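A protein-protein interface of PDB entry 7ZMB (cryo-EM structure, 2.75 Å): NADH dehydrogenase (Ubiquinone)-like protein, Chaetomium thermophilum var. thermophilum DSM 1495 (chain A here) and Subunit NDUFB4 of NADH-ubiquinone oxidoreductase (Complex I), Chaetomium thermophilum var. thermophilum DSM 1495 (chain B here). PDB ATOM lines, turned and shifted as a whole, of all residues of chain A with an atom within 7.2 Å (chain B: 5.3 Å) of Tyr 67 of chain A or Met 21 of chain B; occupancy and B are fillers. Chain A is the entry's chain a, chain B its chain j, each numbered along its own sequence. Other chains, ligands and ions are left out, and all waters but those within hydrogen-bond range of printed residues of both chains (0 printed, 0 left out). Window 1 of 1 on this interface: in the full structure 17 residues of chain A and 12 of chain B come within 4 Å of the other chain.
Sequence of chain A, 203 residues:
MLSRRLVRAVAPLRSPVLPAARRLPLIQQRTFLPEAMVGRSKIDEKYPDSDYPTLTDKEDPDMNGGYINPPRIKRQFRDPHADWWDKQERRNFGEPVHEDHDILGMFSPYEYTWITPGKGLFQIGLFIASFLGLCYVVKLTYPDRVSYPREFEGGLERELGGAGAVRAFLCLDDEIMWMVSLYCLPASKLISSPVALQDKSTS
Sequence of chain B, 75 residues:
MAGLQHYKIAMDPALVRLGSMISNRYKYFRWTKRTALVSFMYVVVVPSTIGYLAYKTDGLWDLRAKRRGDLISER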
ATOM      1  N   GLU A  59     -12.942 -25.547  16.418  1.00  0.00           N
ATOM      2  CA  GLU A  59     -13.215 -24.263  15.788  1.00  0.00           C
ATOM      3  C   GLU A  59     -14.611 -23.726  16.060  1.00  0.00           C
ATOM      4  O   GLU A  59     -14.803 -22.509  16.026  1.00  0.00           O
ATOM      5  CB  GLU A  59     -13.012 -24.360  14.272  1.00  0.00           C
ATOM      6  CG  GLU A  59     -13.789 -25.487  13.619  1.00  0.00           C
ATOM      7  CD  GLU A  59     -13.340 -25.757  12.197  1.00  0.00           C
ATOM      8  OE1 GLU A  59     -12.537 -24.962  11.664  1.00  0.00           O
ATOM      9  OE2 GLU A  59     -13.790 -26.765  11.612  1.00  0.00           O
ATOM     10  N   ASP A  60     -15.586 -24.593  16.329  1.00  0.00           N
ATOM     11  CA  ASP A  60     -16.961 -24.184  16.609  1.00  0.00           C
ATOM     12  C   ASP A  60     -17.434 -24.864  17.888  1.00  0.00           C
ATOM     13  O   ASP A  60     -18.321 -25.724  17.860  1.00  0.00           O
ATOM     14  CB  ASP A  60     -17.880 -24.522  15.434  1.00  0.00           C
ATOM     15  CG  ASP A  60     -19.120 -23.642  15.382  1.00  0.00           C
ATOM     16  OD1 ASP A  60     -19.207 -22.675  16.170  1.00  0.00           O
ATOM     17  OD2 ASP A  60     -20.007 -23.916  14.546  1.00  0.00           O
ATOM     18  N   PRO A  61     -16.853 -24.501  19.035  1.00  0.00           N
ATOM     19  CA  PRO A  61     -17.292 -25.123  20.293  1.00  0.00           C
ATOM     20  C   PRO A  61     -18.737 -24.820  20.646  1.00  0.00           C
ATOM     21  O   PRO A  61     -19.405 -25.649  21.275  1.00  0.00           O
ATOM     22  CB  PRO A  61     -16.316 -24.538  21.321  1.00  0.00           C
ATOM     23  CG  PRO A  61     -15.933 -23.219  20.750  1.00  0.00           C
ATOM     24  CD  PRO A  61     -15.865 -23.432  19.266  1.00  0.00           C
ATOM     25  N   ASP A  62     -19.241 -23.652  20.258  1.00  0.00           N
ATOM     26  CA  ASP A  62     -20.591 -23.231  20.604  1.00  0.00           C
ATOM     27  C   ASP A  62     -21.625 -23.576  19.542  1.00  0.00           C
ATOM     28  O   ASP A  62     -22.795 -23.221  19.710  1.00  0.00           O
ATOM     29  CB  ASP A  62     -20.616 -21.723  20.869  1.00  0.00           C
ATOM     30  CG  ASP A  62     -19.516 -21.280  21.809  1.00  0.00           C
ATOM     31  OD1 ASP A  62     -19.145 -22.068  22.703  1.00  0.00           O
ATOM     32  OD2 ASP A  62     -19.019 -20.146  21.652  1.00  0.00           O
ATOM     33  N   MET A  63     -21.223 -24.241  18.460  1.00  0.00           N
ATOM     34  CA  MET A  63     -22.133 -24.675  17.399  1.00  0.00           C
ATOM     35  C   MET A  63     -22.812 -23.499  16.708  1.00  0.00           C
ATOM     36  O   MET A  63     -23.940 -23.615  16.228  1.00  0.00           O
ATOM     37  CB  MET A  63     -23.183 -25.649  17.930  1.00  0.00           C
ATOM     38  CG  MET A  63     -22.613 -26.962  18.365  1.00  0.00           C
ATOM     39  SD  MET A  63     -23.853 -28.080  18.992  1.00  0.00           S
ATOM     40  CE  MET A  63     -22.795 -29.418  19.467  1.00  0.00           C
ATOM     41  N   ASN A  64     -22.137 -22.360  16.646  1.00  0.00           N
ATOM     42  CA  ASN A  64     -22.694 -21.179  16.010  1.00  0.00           C
ATOM     43  C   ASN A  64     -21.855 -20.678  14.840  1.00  0.00           C
ATOM     44  O   ASN A  64     -21.842 -19.475  14.570  1.00  0.00           O
ATOM     45  CB  ASN A  64     -22.914 -20.088  17.059  1.00  0.00           C
ATOM     46  CG  ASN A  64     -21.631 -19.612  17.703  1.00  0.00           C
ATOM     47  OD1 ASN A  64     -20.533 -19.990  17.308  1.00  0.00           O
ATOM     48  ND2 ASN A  64     -21.770 -18.766  18.711  1.00  0.00           N
ATOM     49  N   GLY A  65     -21.172 -21.571  14.132  1.00  0.00           N
ATOM     50  CA  GLY A  65     -20.471 -21.205  12.919  1.00  0.00           C
ATOM     51  C   GLY A  65     -19.170 -20.465  13.107  1.00  0.00           C
ATOM     52  O   GLY A  65     -18.715 -19.793  12.179  1.00  0.00           O
ATOM     53  N   GLY A  66     -18.545 -20.572  14.274  1.00  0.00           N
ATOM     54  CA  GLY A  66     -17.366 -19.780  14.550  1.00  0.00           C
ATOM     55  C   GLY A  66     -17.657 -18.340  14.897  1.00  0.00           C
ATOM     56  O   GLY A  66     -16.854 -17.458  14.582  1.00  0.00           O
ATOM     57  N   TYR A  67     -18.795 -18.073  15.524  1.00  0.00           N
ATOM     58  CA  TYR A  67     -19.118 -16.720  15.949  1.00  0.00           C
ATOM     59  C   TYR A  67     -18.211 -16.296  17.100  1.00  0.00           C
ATOM     60  O   TYR A  67     -18.080 -17.002  18.102  1.00  0.00           O
ATOM     61  CB  TYR A  67     -20.588 -16.650  16.365  1.00  0.00           C
ATOM     62  CG  TYR A  67     -21.039 -15.312  16.887  1.00  0.00           C
ATOM     63  CD1 TYR A  67     -21.499 -14.325  16.024  1.00  0.00           C
ATOM     64  CD2 TYR A  67     -21.021 -15.038  18.241  1.00  0.00           C
ATOM     65  CE1 TYR A  67     -21.923 -13.098  16.505  1.00  0.00           C
ATOM     66  CE2 TYR A  67     -21.433 -13.822  18.729  1.00  0.00           C
ATOM     67  CZ  TYR A  67     -21.885 -12.853  17.862  1.00  0.00           C
ATOM     68  OH  TYR A  67     -22.302 -11.639  18.361  1.00  0.00           O
ATOM     69  N   ILE A  68     -17.590 -15.134  16.955  1.00  0.00           N
ATOM     70  CA  ILE A  68     -16.678 -14.611  17.966  1.00  0.00           C
ATOM     71  C   ILE A  68     -17.509 -14.012  19.089  1.00  0.00           C
ATOM     72  O   ILE A  68     -18.334 -13.123  18.857  1.00  0.00           O
ATOM     73  CB  ILE A  68     -15.719 -13.569  17.372  1.00  0.00           C
ATOM     74  CG1 ILE A  68     -14.708 -14.246  16.448  1.00  0.00           C
ATOM     75  CG2 ILE A  68     -15.009 -12.809  18.480  1.00  0.00           C
ATOM     76  CD1 ILE A  68     -13.869 -15.301  17.134  1.00  0.00           C
ATOM     77  N   ASN A  69     -17.291 -14.494  20.308  1.00  0.00           N
ATOM     78  CA  ASN A  69     -18.129 -14.113  21.431  1.00  0.00           C
ATOM     79  C   ASN A  69     -17.322 -13.296  22.427  1.00  0.00           C
ATOM     80  O   ASN A  69     -16.326 -13.799  22.966  1.00  0.00           O
ATOM     81  CB  ASN A  69     -18.704 -15.353  22.107  1.00  0.00           C
ATOM     82  CG  ASN A  69     -20.149 -15.181  22.478  1.00  0.00           C
ATOM     83  OD1 ASN A  69     -20.586 -14.080  22.762  1.00  0.00           O
ATOM     84  ND2 ASN A  69     -20.902 -16.276  22.482  1.00  0.00           N
ATOM     85  N   PRO A  70     -17.701 -12.052  22.701  1.00  0.00           N
ATOM     86  CA  PRO A  70     -16.998 -11.265  23.712  1.00  0.00           C
ATOM     87  C   PRO A  70     -17.323 -11.775  25.104  1.00  0.00           C
ATOM     88  O   PRO A  70     -18.216 -12.621  25.265  1.00  0.00           O
ATOM     89  CB  PRO A  70     -17.551  -9.851  23.489  1.00  0.00           C
ATOM     90  CG  PRO A  70     -18.911 -10.082  23.008  1.00  0.00           C
ATOM     91  CD  PRO A  70     -18.850 -11.317  22.146  1.00  0.00           C
ATOM     92  N   PRO A  96     -18.790  -4.987  19.385  1.00  0.00           N
ATOM     93  CA  PRO A  96     -19.162  -6.399  19.278  1.00  0.00           C
ATOM     94  C   PRO A  96     -20.147  -6.786  20.369  1.00  0.00           C
ATOM     95  O   PRO A  96     -20.280  -6.117  21.394  1.00  0.00           O
ATOM     96  CB  PRO A  96     -17.827  -7.138  19.434  1.00  0.00           C
ATOM     97  CG  PRO A  96     -16.875  -6.125  19.982  1.00  0.00           C
ATOM     98  CD  PRO A  96     -17.336  -4.805  19.468  1.00  0.00           C
ATOM     99  N   VAL A  97     -20.858  -7.878  20.128  1.00  0.00           N
ATOM    100  CA  VAL A  97     -22.027  -8.232  20.920  1.00  0.00           C
ATOM    101  C   VAL A  97     -22.001  -9.724  21.210  1.00  0.00           C
ATOM    102  O   VAL A  97     -21.611 -10.530  20.357  1.00  0.00           O
ATOM    103  CB  VAL A  97     -23.327  -7.835  20.188  1.00  0.00           C
ATOM    104  CG1 VAL A  97     -23.521  -6.332  20.216  1.00  0.00           C
ATOM    105  CG2 VAL A  97     -23.294  -8.312  18.766  1.00  0.00           C
ATOM    106  N   HIS A  98     -22.405 -10.089  22.421  1.00  0.00           N
ATOM    107  CA  HIS A  98     -22.581 -11.484  22.786  1.00  0.00           C
ATOM    108  C   HIS A  98     -23.829 -12.057  22.119  1.00  0.00           C
ATOM    109  O   HIS A  98     -24.765 -11.337  21.776  1.00  0.00           O
ATOM    110  CB  HIS A  98     -22.690 -11.619  24.302  1.00  0.00           C
ATOM    111  CG  HIS A  98     -22.422 -12.996  24.813  1.00  0.00           C
ATOM    112  ND1 HIS A  98     -23.336 -14.020  24.708  1.00  0.00           N
ATOM    113  CD2 HIS A  98     -21.345 -13.518  25.443  1.00  0.00           C
ATOM    114  CE1 HIS A  98     -22.830 -15.116  25.240  1.00  0.00           C
ATOM    115  NE2 HIS A  98     -21.622 -14.839  25.694  1.00  0.00           N
ATOM    116  N   GLU A  99     -23.843 -13.380  21.943  1.00  0.00           N
ATOM    117  CA  GLU A  99     -25.055 -14.016  21.440  1.00  0.00           C
ATOM    118  C   GLU A  99     -26.200 -13.969  22.440  1.00  0.00           C
ATOM    119  O   GLU A  99     -27.337 -14.284  22.074  1.00  0.00           O
ATOM    120  CB  GLU A  99     -24.776 -15.457  21.024  1.00  0.00           C
ATOM    121  CG  GLU A  99     -24.723 -16.453  22.137  1.00  0.00           C
ATOM    122  CD  GLU A  99     -23.917 -17.678  21.748  1.00  0.00           C
ATOM    123  OE1 GLU A  99     -22.705 -17.712  22.046  1.00  0.00           O
ATOM    124  OE2 GLU A  99     -24.492 -18.596  21.130  1.00  0.00           O
ATOM    125  N   ASP A 100     -25.928 -13.588  23.686  1.00  0.00           N
ATOM    126  CA  ASP A 100     -26.955 -13.254  24.658  1.00  0.00           C
ATOM    127  C   ASP A 100     -27.152 -11.748  24.772  1.00  0.00           C
ATOM    128  O   ASP A 100     -27.493 -11.247  25.847  1.00  0.00           O
ATOM    129  CB  ASP A 100     -26.609 -13.855  26.018  1.00  0.00           C
ATOM    130  CG  ASP A 100     -26.842 -15.349  26.066  1.00  0.00           C
ATOM    131  OD1 ASP A 100     -27.184 -15.934  25.021  1.00  0.00           O
ATOM    132  OD2 ASP A 100     -26.690 -15.943  27.152  1.00  0.00           O
ATOM    133  N   HIS A 101     -26.916 -11.019  23.681  1.00  0.00           N
ATOM    134  CA  HIS A 101     -27.066  -9.537  23.698  1.00  0.00           C
ATOM    135  C   HIS A 101     -28.449  -9.174  24.226  1.00  0.00           C
ATOM    136  O   HIS A 101     -28.541  -8.180  24.965  1.00  0.00           O
ATOM    137  CB  HIS A 101     -26.832  -8.961  22.294  1.00  0.00           C
ATOM    138  CG  HIS A 101     -27.244  -7.539  22.103  1.00  0.00           C
ATOM    139  ND1 HIS A 101     -26.329  -6.512  22.007  1.00  0.00           N
ATOM    140  CD2 HIS A 101     -28.459  -6.967  21.961  1.00  0.00           C
ATOM    141  CE1 HIS A 101     -26.963  -5.371  21.833  1.00  0.00           C
ATOM    142  NE2 HIS A 101     -28.272  -5.623  21.804  1.00  0.00           N
ATOM    143  N   ALA B  14     -22.387  -5.380  13.943  1.00  0.00           N
ATOM    144  CA  ALA B  14     -22.394  -6.344  15.033  1.00  0.00           C
ATOM    145  C   ALA B  14     -23.796  -6.886  15.269  1.00  0.00           C
ATOM    146  O   ALA B  14     -23.980  -8.093  15.467  1.00  0.00           O
ATOM    147  CB  ALA B  14     -21.844  -5.702  16.306  1.00  0.00           C
ATOM    148  N   ARG B  17     -24.629  -8.922  12.076  1.00  0.00           N
ATOM    149  CA  ARG B  17     -24.004 -10.238  12.047  1.00  0.00           C
ATOM    150  C   ARG B  17     -24.532 -11.147  13.145  1.00  0.00           C
ATOM    151  O   ARG B  17     -24.560 -12.367  12.963  1.00  0.00           O
ATOM    152  CB  ARG B  17     -22.481 -10.111  12.132  1.00  0.00           C
ATOM    153  CG  ARG B  17     -21.924  -9.809  13.505  1.00  0.00           C
ATOM    154  CD  ARG B  17     -20.417  -9.656  13.449  1.00  0.00           C
ATOM    155  NE  ARG B  17     -20.019  -8.559  12.573  1.00  0.00           N
ATOM    156  CZ  ARG B  17     -18.767  -8.322  12.196  1.00  0.00           C
ATOM    157  NH1 ARG B  17     -18.496  -7.301  11.396  1.00  0.00           N
ATOM    158  NH2 ARG B  17     -17.786  -9.106  12.621  1.00  0.00           N
ATOM    159  N   LEU B  18     -24.960 -10.586  14.274  1.00  0.00           N
ATOM    160  CA  LEU B  18     -25.582 -11.405  15.309  1.00  0.00           C
ATOM    161  C   LEU B  18     -26.888 -12.020  14.821  1.00  0.00           C
ATOM    162  O   LEU B  18     -27.207 -13.164  15.161  1.00  0.00           O
ATOM    163  CB  LEU B  18     -25.805 -10.573  16.568  1.00  0.00           C
ATOM    164  CG  LEU B  18     -26.396 -11.283  17.783  1.00  0.00           C
ATOM    165  CD1 LEU B  18     -25.494 -12.372  18.265  1.00  0.00           C
ATOM    166  CD2 LEU B  18     -26.590 -10.268  18.874  1.00  0.00           C
ATOM    167  N   GLY B  19     -27.660 -11.275  14.030  1.00  0.00           N
ATOM    168  CA  GLY B  19     -28.849 -11.838  13.421  1.00  0.00           C
ATOM    169  C   GLY B  19     -28.546 -12.944  12.432  1.00  0.00           C
ATOM    170  O   GLY B  19     -29.316 -13.901  12.314  1.00  0.00           O
ATOM    171  N   SER B  20     -27.434 -12.829  11.705  1.00  0.00           N
ATOM    172  CA  SER B  20     -27.061 -13.879  10.763  1.00  0.00           C
ATOM    173  C   SER B  20     -26.774 -15.191  11.476  1.00  0.00           C
ATOM    174  O   SER B  20     -27.200 -16.256  11.021  1.00  0.00           O
ATOM    175  CB  SER B  20     -25.847 -13.448   9.948  1.00  0.00           C
ATOM    176  OG  SER B  20     -25.454 -14.472   9.055  1.00  0.00           O
ATOM    177  N   MET B  21     -26.050 -15.135  12.594  1.00  0.00           N
ATOM    178  CA  MET B  21     -25.703 -16.358  13.308  1.00  0.00           C
ATOM    179  C   MET B  21     -26.932 -16.992  13.946  1.00  0.00           C
ATOM    180  O   MET B  21     -27.097 -18.216  13.908  1.00  0.00           O
ATOM    181  CB  MET B  21     -24.631 -16.062  14.360  1.00  0.00           C
ATOM    182  CG  MET B  21     -24.211 -17.270  15.171  1.00  0.00           C
ATOM    183  SD  MET B  21     -24.973 -17.352  16.801  1.00  0.00           S
ATOM    184  CE  MET B  21     -24.622 -15.707  17.401  1.00  0.00           C
ATOM    185  N   ILE B  22     -27.803 -16.181  14.549  1.00  0.00           N
ATOM    186  CA  ILE B  22     -29.030 -16.727  15.121  1.00  0.00           C
ATOM    187  C   ILE B  22     -29.873 -17.367  14.029  1.00  0.00           C
ATOM    188  O   ILE B  22     -30.472 -18.431  14.222  1.00  0.00           O
ATOM    189  CB  ILE B  22     -29.818 -15.636  15.870  1.00  0.00           C
ATOM    190  CG1 ILE B  22     -28.988 -15.024  16.992  1.00  0.00           C
ATOM    191  CG2 ILE B  22     -31.079 -16.213  16.460  1.00  0.00           C
ATOM    192  CD1 ILE B  22     -28.280 -16.007  17.811  1.00  0.00           C
ATOM    193  N   SER B  23     -29.926 -16.727  12.861  1.00  0.00           N
ATOM    194  CA  SER B  23     -30.645 -17.286  11.726  1.00  0.00           C
ATOM    195  C   SER B  23     -30.045 -18.612  11.292  1.00  0.00           C
ATOM    196  O   SER B  23     -30.768 -19.580  11.044  1.00  0.00           O
ATOM    197  CB  SER B  23     -30.622 -16.294  10.567  1.00  0.00           C
ATOM    198  OG  SER B  23     -31.280 -16.819   9.438  1.00  0.00           O
ATOM    199  N   ASN B  24     -28.719 -18.678  11.207  1.00  0.00           N
ATOM    200  CA  ASN B  24     -28.025 -19.799  10.600  1.00  0.00           C
ATOM    201  C   ASN B  24     -27.464 -20.785  11.613  1.00  0.00           C
ATOM    202  O   ASN B  24     -26.768 -21.722  11.216  1.00  0.00           O
ATOM    203  CB  ASN B  24     -26.898 -19.292   9.706  1.00  0.00           C
ATOM    204  CG  ASN B  24     -27.386 -18.352   8.626  1.00  0.00           C
ATOM    205  OD1 ASN B  24     -26.786 -17.313   8.383  1.00  0.00           O
ATOM    206  ND2 ASN B  24     -28.474 -18.721   7.967  1.00  0.00           N
ATOM    207  N   ARG B  25     -27.749 -20.605  12.907  1.00  0.00           N
ATOM    208  CA  ARG B  25     -27.233 -21.532  13.908  1.00  0.00           C
ATOM    209  C   ARG B  25     -27.650 -22.977  13.656  1.00  0.00           C
ATOM    210  O   ARG B  25     -26.922 -23.894  14.050  1.00  0.00           O
ATOM    211  CB  ARG B  25     -27.654 -21.103  15.326  1.00  0.00           C
ATOM    212  CG  ARG B  25     -27.044 -22.011  16.382  1.00  0.00           C
ATOM    213  CD  ARG B  25     -27.322 -21.718  17.848  1.00  0.00           C
ATOM    214  NE  ARG B  25     -26.769 -20.464  18.334  1.00  0.00           N
ATOM    215  CZ  ARG B  25     -27.471 -19.410  18.723  1.00  0.00           C
ATOM    216  NH1 ARG B  25     -28.797 -19.418  18.699  1.00  0.00           N
ATOM    217  NH2 ARG B  25     -26.822 -18.346  19.163  1.00  0.00           N
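The side-chain carboxylate (OE2) of Glu 99 of chain A is in salt-bridge range of the guanidinium group (NH2) of Arg 25 of chain B (3.1 Å).
A ring nitrogen (NE2) of His 98 of chain A sits close to the side-chain amide oxygen (OD1) of Asn 69 of chain A. N of Asn 64 of chain A lies within hydrogen-bond range of OD1 of Asp 60 of chain A, 3.0 Å away. The backbone NH (N) of Asp 100 of chain A is in hydrogen-bond range of a ring nitrogen (ND1) of His 98 of chain A (2.8 Å). The side-chain amide oxygen (OD1) of Asn 64 of chain A lies within hydrogen-bond range of the backbone NH (N) of Tyr 67 of chain A. N of Met 63 of chain A lies within hydrogen-bond range of OD1 of Asp 60 of chain A (3.4 Å). The guanidinium group (NH2) of Arg 25 of chain B lies within hydrogen-bond range of the side-chain sulfur (SD) of Met 21 of chain B, at 3.2 Å.
Of chain B, only Leu 18 and Met 21 come within 4 Å of Tyr 67 of chain A. Printed residues of chain A within 4 Å of Met 21 of chain B: Asn 64 (3.3 Å), Tyr 67 (3.6 Å) and Glu 99 (3.6 Å). Of the printed residues of chain A, Leu 18 of chain B touches Tyr 67, Val 97, His 98, Glu 99 and His 101. Of the printed residues of chain A, Ala 14 of chain B touches Val 97 (3.4 Å). Printed residues of chain B within 4 Å of Glu 99 of chain A: Leu 18, Met 21 and Arg 25. The nearest printed residue of chain B that does not touch Glu 99 of chain A is Ile 22 of chain B (4.7 Å).
Of the 10 printed residues of chain B, 4 touch a printed residue of chain A. Hydrophobic or aromatic side chains of chain B that line the printed part of chain A: Ala 14, Leu 18 and Met 21. Hydrophobic or aromatic side chains of chain A within 4 Å of the printed part of chain B: Tyr 67, Val 97 and His 101. Among the printed residues, 11 pairs touch across the chains.
Among the printed residues, pairs that only touch across the chains: Tyr 67 of chain A with Leu 18 of chain B (3.3 Å), Asn 64 of chain A with Met 21 of chain B (3.3 Å), Val 97 of chain A with Ala 14 of chain B (3.4 Å), Met 63 of chain A with Arg 25 of chain B (3.5 Å), His 98 of chain A with Leu 18 of chain B (3.6 Å), Glu 99 of chain A with Leu 18 of chain B (3.6 Å), Glu 99 of chain A with Met 21 of chain B (3.6 Å), Tyr 67 of chain A with Met 21 of chain B (3.6 Å), His 101 of chain A with Leu 18 of chain B (3.7 Å) and Val 97 of chain A with Leu 18 of chain B (3.8 Å).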
